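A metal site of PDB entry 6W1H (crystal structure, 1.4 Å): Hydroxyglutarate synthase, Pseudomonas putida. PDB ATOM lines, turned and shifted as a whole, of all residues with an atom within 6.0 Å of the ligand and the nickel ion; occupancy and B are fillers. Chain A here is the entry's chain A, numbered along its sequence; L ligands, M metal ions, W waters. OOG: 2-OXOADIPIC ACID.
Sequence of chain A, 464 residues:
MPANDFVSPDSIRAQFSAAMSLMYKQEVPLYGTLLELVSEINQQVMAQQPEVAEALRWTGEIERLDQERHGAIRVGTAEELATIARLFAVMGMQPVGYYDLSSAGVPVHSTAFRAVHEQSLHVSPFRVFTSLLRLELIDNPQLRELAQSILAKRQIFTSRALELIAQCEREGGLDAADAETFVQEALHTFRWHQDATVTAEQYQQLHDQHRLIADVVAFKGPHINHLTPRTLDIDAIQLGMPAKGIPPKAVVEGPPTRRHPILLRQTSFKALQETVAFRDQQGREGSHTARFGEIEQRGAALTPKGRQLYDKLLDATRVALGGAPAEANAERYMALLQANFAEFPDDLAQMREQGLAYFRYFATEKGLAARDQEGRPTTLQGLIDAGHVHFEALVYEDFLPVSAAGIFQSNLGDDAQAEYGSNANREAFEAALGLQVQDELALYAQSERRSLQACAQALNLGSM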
ATOM      1  N   HIS A  70      -8.902  21.306  32.453  1.00  0.00           N
ATOM      2  CA  HIS A  70      -9.814  21.355  31.311  1.00  0.00           C
ATOM      3  C   HIS A  70      -9.061  20.834  30.083  1.00  0.00           C
ATOM      4  O   HIS A  70      -7.838  20.911  30.013  1.00  0.00           O
ATOM      5  CB  HIS A  70     -10.505  22.704  31.064  1.00  0.00           C
ATOM      6  CG  HIS A  70      -9.754  23.710  30.247  1.00  0.00           C
ATOM      7  ND1 HIS A  70      -9.301  24.895  30.782  1.00  0.00           N
ATOM      8  CD2 HIS A  70      -9.479  23.764  28.923  1.00  0.00           C
ATOM      9  CE1 HIS A  70      -8.731  25.625  29.836  1.00  0.00           C
ATOM     10  NE2 HIS A  70      -8.835  24.963  28.695  1.00  0.00           N
ATOM     11  N   GLY A  71      -9.792  20.237  29.175  1.00  0.00           N
ATOM     12  CA  GLY A  71      -9.277  19.912  27.868  1.00  0.00           C
ATOM     13  C   GLY A  71     -10.037  20.677  26.815  1.00  0.00           C
ATOM     14  O   GLY A  71     -11.135  21.189  27.074  1.00  0.00           O
ATOM     15  N   ALA A  72      -9.473  20.716  25.604  1.00  0.00           N
ATOM     16  CA  ALA A  72     -10.157  21.315  24.466  1.00  0.00           C
ATOM     17  C   ALA A  72      -9.970  20.405  23.271  1.00  0.00           C
ATOM     18  O   ALA A  72      -8.866  19.936  23.013  1.00  0.00           O
ATOM     19  CB  ALA A  72      -9.566  22.688  24.136  1.00  0.00           C
ATOM     20  N   ILE A  73     -11.065  20.166  22.538  1.00  0.00           N
ATOM     21  CA  ILE A  73     -11.052  19.312  21.375  1.00  0.00           C
ATOM     22  C   ILE A  73     -11.930  19.946  20.303  1.00  0.00           C
ATOM     23  O   ILE A  73     -12.776  20.791  20.581  1.00  0.00           O
ATOM     24  CB  ILE A  73     -11.555  17.878  21.656  1.00  0.00           C
ATOM     25  CG1 ILE A  73     -12.993  17.902  22.156  1.00  0.00           C
ATOM     26  CG2 ILE A  73     -10.643  17.210  22.659  1.00  0.00           C
ATOM     27  CD1 ILE A  73     -13.606  16.520  22.317  1.00  0.00           C
ATOM     28  N   ARG A  74     -11.704  19.497  19.068  1.00  0.00           N
ATOM     29  CA  ARG A  74     -12.487  19.939  17.908  1.00  0.00           C
ATOM     30  C   ARG A  74     -12.943  18.718  17.127  1.00  0.00           C
ATOM     31  O   ARG A  74     -12.150  17.797  16.895  1.00  0.00           O
ATOM     32  CB  ARG A  74     -11.658  20.833  16.999  1.00  0.00           C
ATOM     33  CG  ARG A  74     -11.158  22.092  17.662  1.00  0.00           C
ATOM     34  CD  ARG A  74      -9.678  22.207  17.540  1.00  0.00           C
ATOM     35  NE  ARG A  74      -9.191  23.492  18.035  1.00  0.00           N
ATOM     36  CZ  ARG A  74      -8.120  24.109  17.545  1.00  0.00           C
ATOM     37  NH1 ARG A  74      -7.424  23.560  16.580  1.00  0.00           N
ATOM     38  NH2 ARG A  74      -7.758  25.268  18.053  1.00  0.00           N
ATOM     39  N   PHE A 129     -13.950  21.544  26.619  1.00  0.00           N
ATOM     40  CA  PHE A 129     -14.524  22.495  25.668  1.00  0.00           C
ATOM     41  C   PHE A 129     -14.463  21.849  24.306  1.00  0.00           C
ATOM     42  O   PHE A 129     -13.384  21.437  23.864  1.00  0.00           O
ATOM     43  CB  PHE A 129     -13.722  23.779  25.692  1.00  0.00           C
ATOM     44  CG  PHE A 129     -14.341  24.915  24.933  1.00  0.00           C
ATOM     45  CD1 PHE A 129     -14.152  25.042  23.557  1.00  0.00           C
ATOM     46  CD2 PHE A 129     -15.104  25.870  25.589  1.00  0.00           C
ATOM     47  CE1 PHE A 129     -14.701  26.121  22.853  1.00  0.00           C
ATOM     48  CE2 PHE A 129     -15.658  26.936  24.895  1.00  0.00           C
ATOM     49  CZ  PHE A 129     -15.439  27.072  23.525  1.00  0.00           C
ATOM     50  N   SER A 131     -15.550  21.958  20.260  1.00  0.00           N
ATOM     51  CA  SER A 131     -15.943  22.768  19.127  1.00  0.00           C
ATOM     52  C   SER A 131     -16.327  21.881  17.949  1.00  0.00           C
ATOM     53  O   SER A 131     -15.669  20.869  17.673  1.00  0.00           O
ATOM     54  CB  SER A 131     -14.790  23.678  18.713  1.00  0.00           C
ATOM     55  OG  SER A 131     -14.531  24.630  19.703  1.00  0.00           O
ATOM     56  N   LEU A 212      -6.828  25.723  11.501  1.00  0.00           N
ATOM     57  CA  LEU A 212      -7.790  24.931  12.256  1.00  0.00           C
ATOM     58  C   LEU A 212      -8.463  23.895  11.371  1.00  0.00           C
ATOM     59  O   LEU A 212      -8.786  22.794  11.835  1.00  0.00           O
ATOM     60  CB  LEU A 212      -8.844  25.825  12.896  1.00  0.00           C
ATOM     61  CG  LEU A 212      -9.796  25.097  13.857  1.00  0.00           C
ATOM     62  CD1 LEU A 212     -10.064  25.922  15.102  1.00  0.00           C
ATOM     63  CD2 LEU A 212     -11.088  24.759  13.151  1.00  0.00           C
ATOM     64  N   ASN A 225      -6.277  19.312  21.976  1.00  0.00           N
ATOM     65  CA  ASN A 225      -5.683  20.571  21.546  1.00  0.00           C
ATOM     66  C   ASN A 225      -4.815  21.136  22.653  1.00  0.00           C
ATOM     67  O   ASN A 225      -3.754  21.693  22.385  1.00  0.00           O
ATOM     68  CB  ASN A 225      -6.767  21.576  21.163  1.00  0.00           C
ATOM     69  CG  ASN A 225      -6.184  22.862  20.655  1.00  0.00           C
ATOM     70  OD1 ASN A 225      -6.009  23.803  21.415  1.00  0.00           O
ATOM     71  ND2 ASN A 225      -5.837  22.890  19.389  1.00  0.00           N
ATOM     72  N   HIS A 226      -5.254  21.028  23.900  1.00  0.00           N
ATOM     73  CA  HIS A 226      -4.442  21.282  25.068  1.00  0.00           C
ATOM     74  C   HIS A 226      -5.187  20.748  26.290  1.00  0.00           C
ATOM     75  O   HIS A 226      -6.391  20.509  26.256  1.00  0.00           O
ATOM     76  CB  HIS A 226      -4.136  22.752  25.199  1.00  0.00           C
ATOM     77  CG  HIS A 226      -5.343  23.624  25.336  1.00  0.00           C
ATOM     78  ND1 HIS A 226      -5.993  24.144  24.239  1.00  0.00           N
ATOM     79  CD2 HIS A 226      -6.047  24.030  26.415  1.00  0.00           C
ATOM     80  CE1 HIS A 226      -7.004  24.901  24.640  1.00  0.00           C
ATOM     81  NE2 HIS A 226      -7.072  24.830  25.958  1.00  0.00           N
ATOM     82  N   THR A 228      -5.267  22.002  30.364  1.00  0.00           N
ATOM     83  CA  THR A 228      -4.907  23.169  31.158  1.00  0.00           C
ATOM     84  C   THR A 228      -5.084  22.855  32.622  1.00  0.00           C
ATOM     85  O   THR A 228      -6.213  22.565  33.050  1.00  0.00           O
ATOM     86  CB  THR A 228      -5.824  24.334  30.766  1.00  0.00           C
ATOM     87  OG1 THR A 228      -5.641  24.535  29.375  1.00  0.00           O
ATOM     88  CG2 THR A 228      -5.496  25.587  31.550  1.00  0.00           C
ATOM     89  N   LEU A 264     -12.052  33.750  34.896  1.00  0.00           N
ATOM     90  CA  LEU A 264     -10.736  33.136  34.939  1.00  0.00           C
ATOM     91  C   LEU A 264      -9.728  34.033  34.234  1.00  0.00           C
ATOM     92  O   LEU A 264     -10.092  34.971  33.521  1.00  0.00           O
ATOM     93  CB  LEU A 264     -10.741  31.750  34.296  1.00  0.00           C
ATOM     94  CG  LEU A 264     -10.995  31.621  32.796  1.00  0.00           C
ATOM     95  CD1 LEU A 264      -9.758  31.927  31.985  1.00  0.00           C
ATOM     96  CD2 LEU A 264     -11.490  30.217  32.479  1.00  0.00           C
ATOM     97  N   GLN A 266      -5.949  33.619  31.991  1.00  0.00           N
ATOM     98  CA  GLN A 266      -5.298  32.605  31.167  1.00  0.00           C
ATOM     99  C   GLN A 266      -4.111  33.182  30.432  1.00  0.00           C
ATOM    100  O   GLN A 266      -4.059  34.366  30.131  1.00  0.00           O
ATOM    101  CB  GLN A 266      -6.303  32.047  30.156  1.00  0.00           C
ATOM    102  CG  GLN A 266      -5.706  31.117  29.092  1.00  0.00           C
ATOM    103  CD  GLN A 266      -5.164  31.871  27.868  1.00  0.00           C
ATOM    104  OE1 GLN A 266      -5.065  33.109  27.866  1.00  0.00           O
ATOM    105  NE2 GLN A 266      -4.807  31.125  26.826  1.00  0.00           N
ATOM    106  N   GLU A 294      -1.320  25.781  27.925  1.00  0.00           N
ATOM    107  CA  GLU A 294      -2.103  26.817  28.559  1.00  0.00           C
ATOM    108  C   GLU A 294      -2.102  26.630  30.072  1.00  0.00           C
ATOM    109  O   GLU A 294      -1.915  25.530  30.592  1.00  0.00           O
ATOM    110  CB  GLU A 294      -3.529  26.725  28.014  1.00  0.00           C
ATOM    111  CG  GLU A 294      -4.525  27.760  28.511  1.00  0.00           C
ATOM    112  CD  GLU A 294      -5.806  27.669  27.727  1.00  0.00           C
ATOM    113  OE1 GLU A 294      -6.640  26.819  28.060  1.00  0.00           O
ATOM    114  OE2 GLU A 294      -5.946  28.395  26.739  1.00  0.00           O
ATOM    115  N   GLU A 296      -4.369  28.351  33.572  1.00  0.00           N
ATOM    116  CA  GLU A 296      -5.475  29.202  33.985  1.00  0.00           C
ATOM    117  C   GLU A 296      -5.568  29.291  35.500  1.00  0.00           C
ATOM    118  O   GLU A 296      -5.080  28.433  36.228  1.00  0.00           O
ATOM    119  CB  GLU A 296      -6.814  28.741  33.391  1.00  0.00           C
ATOM    120  CG  GLU A 296      -7.395  27.488  33.992  1.00  0.00           C
ATOM    121  CD  GLU A 296      -8.566  26.938  33.181  1.00  0.00           C
ATOM    122  OE1 GLU A 296      -9.050  27.599  32.238  1.00  0.00           O
ATOM    123  OE2 GLU A 296      -9.009  25.838  33.483  1.00  0.00           O
ATOM    124  N   PHE A 399     -15.898  29.076  30.434  1.00  0.00           N
ATOM    125  CA  PHE A 399     -14.802  29.571  29.608  1.00  0.00           C
ATOM    126  C   PHE A 399     -15.085  30.988  29.103  1.00  0.00           C
ATOM    127  O   PHE A 399     -16.237  31.375  28.926  1.00  0.00           O
ATOM    128  CB  PHE A 399     -14.586  28.607  28.414  1.00  0.00           C
ATOM    129  CG  PHE A 399     -14.224  27.236  28.836  1.00  0.00           C
ATOM    130  CD1 PHE A 399     -15.204  26.309  29.159  1.00  0.00           C
ATOM    131  CD2 PHE A 399     -12.888  26.866  28.932  1.00  0.00           C
ATOM    132  CE1 PHE A 399     -14.840  25.024  29.577  1.00  0.00           C
ATOM    133  CE2 PHE A 399     -12.535  25.610  29.343  1.00  0.00           C
ATOM    134  CZ  PHE A 399     -13.504  24.677  29.653  1.00  0.00           C
ATOM    135  N   LEU A 400     -14.039  31.759  28.942  1.00  0.00           N
ATOM    136  CA  LEU A 400     -14.198  33.147  28.486  1.00  0.00           C
ATOM    137  C   LEU A 400     -14.892  33.249  27.137  1.00  0.00           C
ATOM    138  O   LEU A 400     -15.771  34.110  27.014  1.00  0.00           O
ATOM    139  CB  LEU A 400     -12.851  33.868  28.505  1.00  0.00           C
ATOM    140  CG  LEU A 400     -12.168  34.017  29.851  1.00  0.00           C
ATOM    141  CD1 LEU A 400     -10.797  34.689  29.639  1.00  0.00           C
ATOM    142  CD2 LEU A 400     -13.010  34.774  30.813  1.00  0.00           C
ATOM    143  N   PRO A 401     -14.515  32.500  26.081  1.00  0.00           N
ATOM    144  CA  PRO A 401     -13.382  31.562  25.943  1.00  0.00           C
ATOM    145  C   PRO A 401     -12.139  32.209  25.314  1.00  0.00           C
ATOM    146  O   PRO A 401     -12.183  33.342  24.823  1.00  0.00           O
ATOM    147  CB  PRO A 401     -13.935  30.535  24.957  1.00  0.00           C
ATOM    148  CG  PRO A 401     -14.772  31.380  24.003  1.00  0.00           C
ATOM    149  CD  PRO A 401     -15.306  32.549  24.826  1.00  0.00           C
ATOM    150  N   VAL A 402     -11.014  31.499  25.282  1.00  0.00           N
ATOM    151  CA  VAL A 402      -9.706  31.951  24.783  1.00  0.00           C
ATOM    152  C   VAL A 402      -9.084  30.779  24.046  1.00  0.00           C
ATOM    153  O   VAL A 402      -9.390  29.713  24.266  1.00  0.00           O
ATOM    154  CB  VAL A 402      -8.818  32.452  25.954  1.00  0.00           C
ATOM    155  CG1 VAL A 402      -8.466  31.359  26.954  1.00  0.00           C
ATOM    156  CG2 VAL A 402      -7.548  33.144  25.465  1.00  0.00           C
ATOM    157  N   SER A 403      -8.270  31.032  23.069  1.00  0.00           N
ATOM    158  CA  SER A 403      -7.605  29.996  22.283  1.00  0.00           C
ATOM    159  C   SER A 403      -6.109  30.016  22.558  1.00  0.00           C
ATOM    160  O   SER A 403      -5.436  31.018  22.282  1.00  0.00           O
ATOM    161  CB  SER A 403      -7.863  30.193  20.784  1.00  0.00           C
ATOM    162  OG  SER A 403      -7.374  29.087  20.023  1.00  0.00           O
ATOM    163  N   ALA A 404      -5.596  28.905  23.083  1.00  0.00           N
ATOM    164  CA  ALA A 404      -4.164  28.805  23.301  1.00  0.00           C
ATOM    165  C   ALA A 404      -3.382  28.884  21.994  1.00  0.00           C
ATOM    166  O   ALA A 404      -2.255  29.390  21.976  1.00  0.00           O
ATOM    167  CB  ALA A 404      -3.823  27.507  24.037  1.00  0.00           C
ATOM    168  N   ALA A 405      -3.954  28.370  20.911  1.00  0.00           N
ATOM    169  CA  ALA A 405      -3.307  28.374  19.603  1.00  0.00           C
ATOM    170  C   ALA A 405      -3.584  29.655  18.824  1.00  0.00           C
ATOM    171  O   ALA A 405      -3.188  29.740  17.665  1.00  0.00           O
ATOM    172  CB  ALA A 405      -3.746  27.152  18.789  1.00  0.00           C
ATOM    173  N   ILE A 407      -6.526  30.990  17.689  1.00  0.00           N
ATOM    174  CA  ILE A 407      -7.450  30.832  16.566  1.00  0.00           C
ATOM    175  C   ILE A 407      -8.488  31.947  16.537  1.00  0.00           C
ATOM    176  O   ILE A 407      -8.856  32.430  15.461  1.00  0.00           O
ATOM    177  CB  ILE A 407      -8.096  29.432  16.610  1.00  0.00           C
ATOM    178  CG1 ILE A 407      -7.047  28.332  16.536  1.00  0.00           C
ATOM    179  CG2 ILE A 407      -9.098  29.272  15.460  1.00  0.00           C
ATOM    180  CD1 ILE A 407      -6.188  28.366  15.285  1.00  0.00           C
ATOM    181  N   PHE A 408      -8.972  32.373  17.703  1.00  0.00           N
ATOM    182  CA  PHE A 408     -10.000  33.407  17.769  1.00  0.00           C
ATOM    183  C   PHE A 408      -9.638  34.436  18.838  1.00  0.00           C
ATOM    184  O   PHE A 408      -8.831  34.181  19.732  1.00  0.00           O
ATOM    185  CB  PHE A 408     -11.389  32.825  18.070  1.00  0.00           C
ATOM    186  CG  PHE A 408     -11.417  31.846  19.214  1.00  0.00           C
ATOM    187  CD1 PHE A 408     -11.553  32.283  20.524  1.00  0.00           C
ATOM    188  CD2 PHE A 408     -11.329  30.485  18.972  1.00  0.00           C
ATOM    189  CE1 PHE A 408     -11.589  31.377  21.572  1.00  0.00           C
ATOM    190  CE2 PHE A 408     -11.352  29.572  20.017  1.00  0.00           C
ATOM    191  CZ  PHE A 408     -11.494  30.020  21.309  1.00  0.00           C
HETATM  192  C2  OOG L   1      -9.829  26.830  22.363  1.00  0.00           C
HETATM  193  C3  OOG L   1     -11.019  26.222  23.077  1.00  0.00           C
HETATM  194  C4  OOG L   1     -11.432  27.071  24.266  1.00  0.00           C
HETATM  195  C6  OOG L   1     -10.434  27.867  26.565  1.00  0.00           C
HETATM  196  O4  OOG L   1     -11.273  28.829  26.584  1.00  0.00           O
HETATM  197  O3  OOG L   1      -9.522  27.733  27.438  1.00  0.00           O
HETATM  198  C5  OOG L   1     -10.499  26.831  25.465  1.00  0.00           C
HETATM  199  C1  OOG L   1      -9.560  26.145  21.015  1.00  0.00           C
HETATM  200  O1  OOG L   1      -8.764  26.608  20.258  1.00  0.00           O
HETATM  201  O2  OOG L   1     -10.231  24.977  20.630  1.00  0.00           O
HETATM  202  O5  OOG L   1      -9.833  25.848  25.596  1.00  0.00           O
HETATM  203 NI    NI M   1      -8.246  26.203  26.964  1.00  0.00          NI
HETATM  204  O   HOH W   1      -6.295  26.411  21.473  1.00  0.00           O
HETATM  205  O   HOH W   2      -7.598  27.752  25.202  1.00  0.00           O
HETATM  206  O   HOH W   3     -11.464  30.444  28.799  1.00  0.00           O
HETATM  207  O   HOH W   4      -8.902  29.379  29.650  1.00  0.00           O
HETATM  208  O   HOH W   5     -12.514  23.586  21.024  1.00  0.00           O
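N of Val 402 sits at hydrogen-bond distance from O4 of the ligand (3.0 Å). The guanidinium group (NH2) of Arg 74 is in salt-bridge range of an oxygen (O1) of the ligand, 2.8 Å away. An oxygen (O1) of the ligand lies within hydrogen-bond range of the side-chain hydroxyl of Ser 403 (2.9 Å).
OE1 of Glu 294 binds the nickel ion (2.0 Å). The nickel ion is bound by an oxygen (O3) of the ligand (2.0 Å). A ring nitrogen (NE2) of His 226 is bound to the nickel ion (2.1 Å). The nickel ion is bound by an oxygen (O5) of the ligand (2.1 Å). NE2 of His 70 binds the nickel ion, at 2.2 Å. The nickel ion is bound by water W2, at 2.4 Å. The nickel ion has six donor atoms within binding distance.
Residues that only touch the ligand: Ala 72 (3.5 Å), Phe 129 (3.4 Å), Phe 399 (3.5 Å), Pro 401 (3.5 Å) and Phe 408 (3.7 Å). Hydrophobic or aromatic side chains within 4 Å of the ligand: His 70, Ala 72, Phe 129, His 226, Phe 399, Pro 401, Val 402 and Phe 408.
Thr 228 touches the nickel ion.
Water W5 lies within hydrogen-bond range of OG of Ser 131 (2.6 Å), O2 of the ligand (2.7 Å) and O of Ile 73 (2.8 Å). Water W3 bridges O4 of the ligand (2.7 Å) and N of Leu 400 (2.9 Å). Water W1 lies within hydrogen-bond range of the side-chain amide oxygen of Asn 225 (2.6 Å), an oxygen (O1) of the ligand (2.8 Å), the backbone NH of Ala 404 (3.0 Å), the backbone NH of Ala 405 (3.1 Å) and the side-chain hydroxyl of Ser 403 (3.2 Å).
O of Phe 129 lies within hydrogen-bond range of N of Ile 73. OE2 of Glu 294 sits at hydrogen-bond distance from NE2 of Gln 266 (3.0 Å). N of Thr 228 lies within hydrogen-bond range of O of His 70 (2.8 Å). The backbone NH (N) of Phe 129 lies within hydrogen-bond range of the backbone carbonyl oxygen (O) of Gly 71, at 2.9 Å. The backbone NH (N) of Asn 225 sits at hydrogen-bond distance from the backbone carbonyl oxygen (O) of Ala 72 (2.9 Å). The backbone NH (N) of Ala 72 is in hydrogen-bond range of the backbone carbonyl oxygen (O) of His 226, at 3.2 Å. OG of Ser 403 sits at hydrogen-bond distance from N of Ile 407, at 3.1 Å. A ring nitrogen (ND1) of His 226 lies within hydrogen-bond range of the side-chain amide oxygen of Asn 225.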
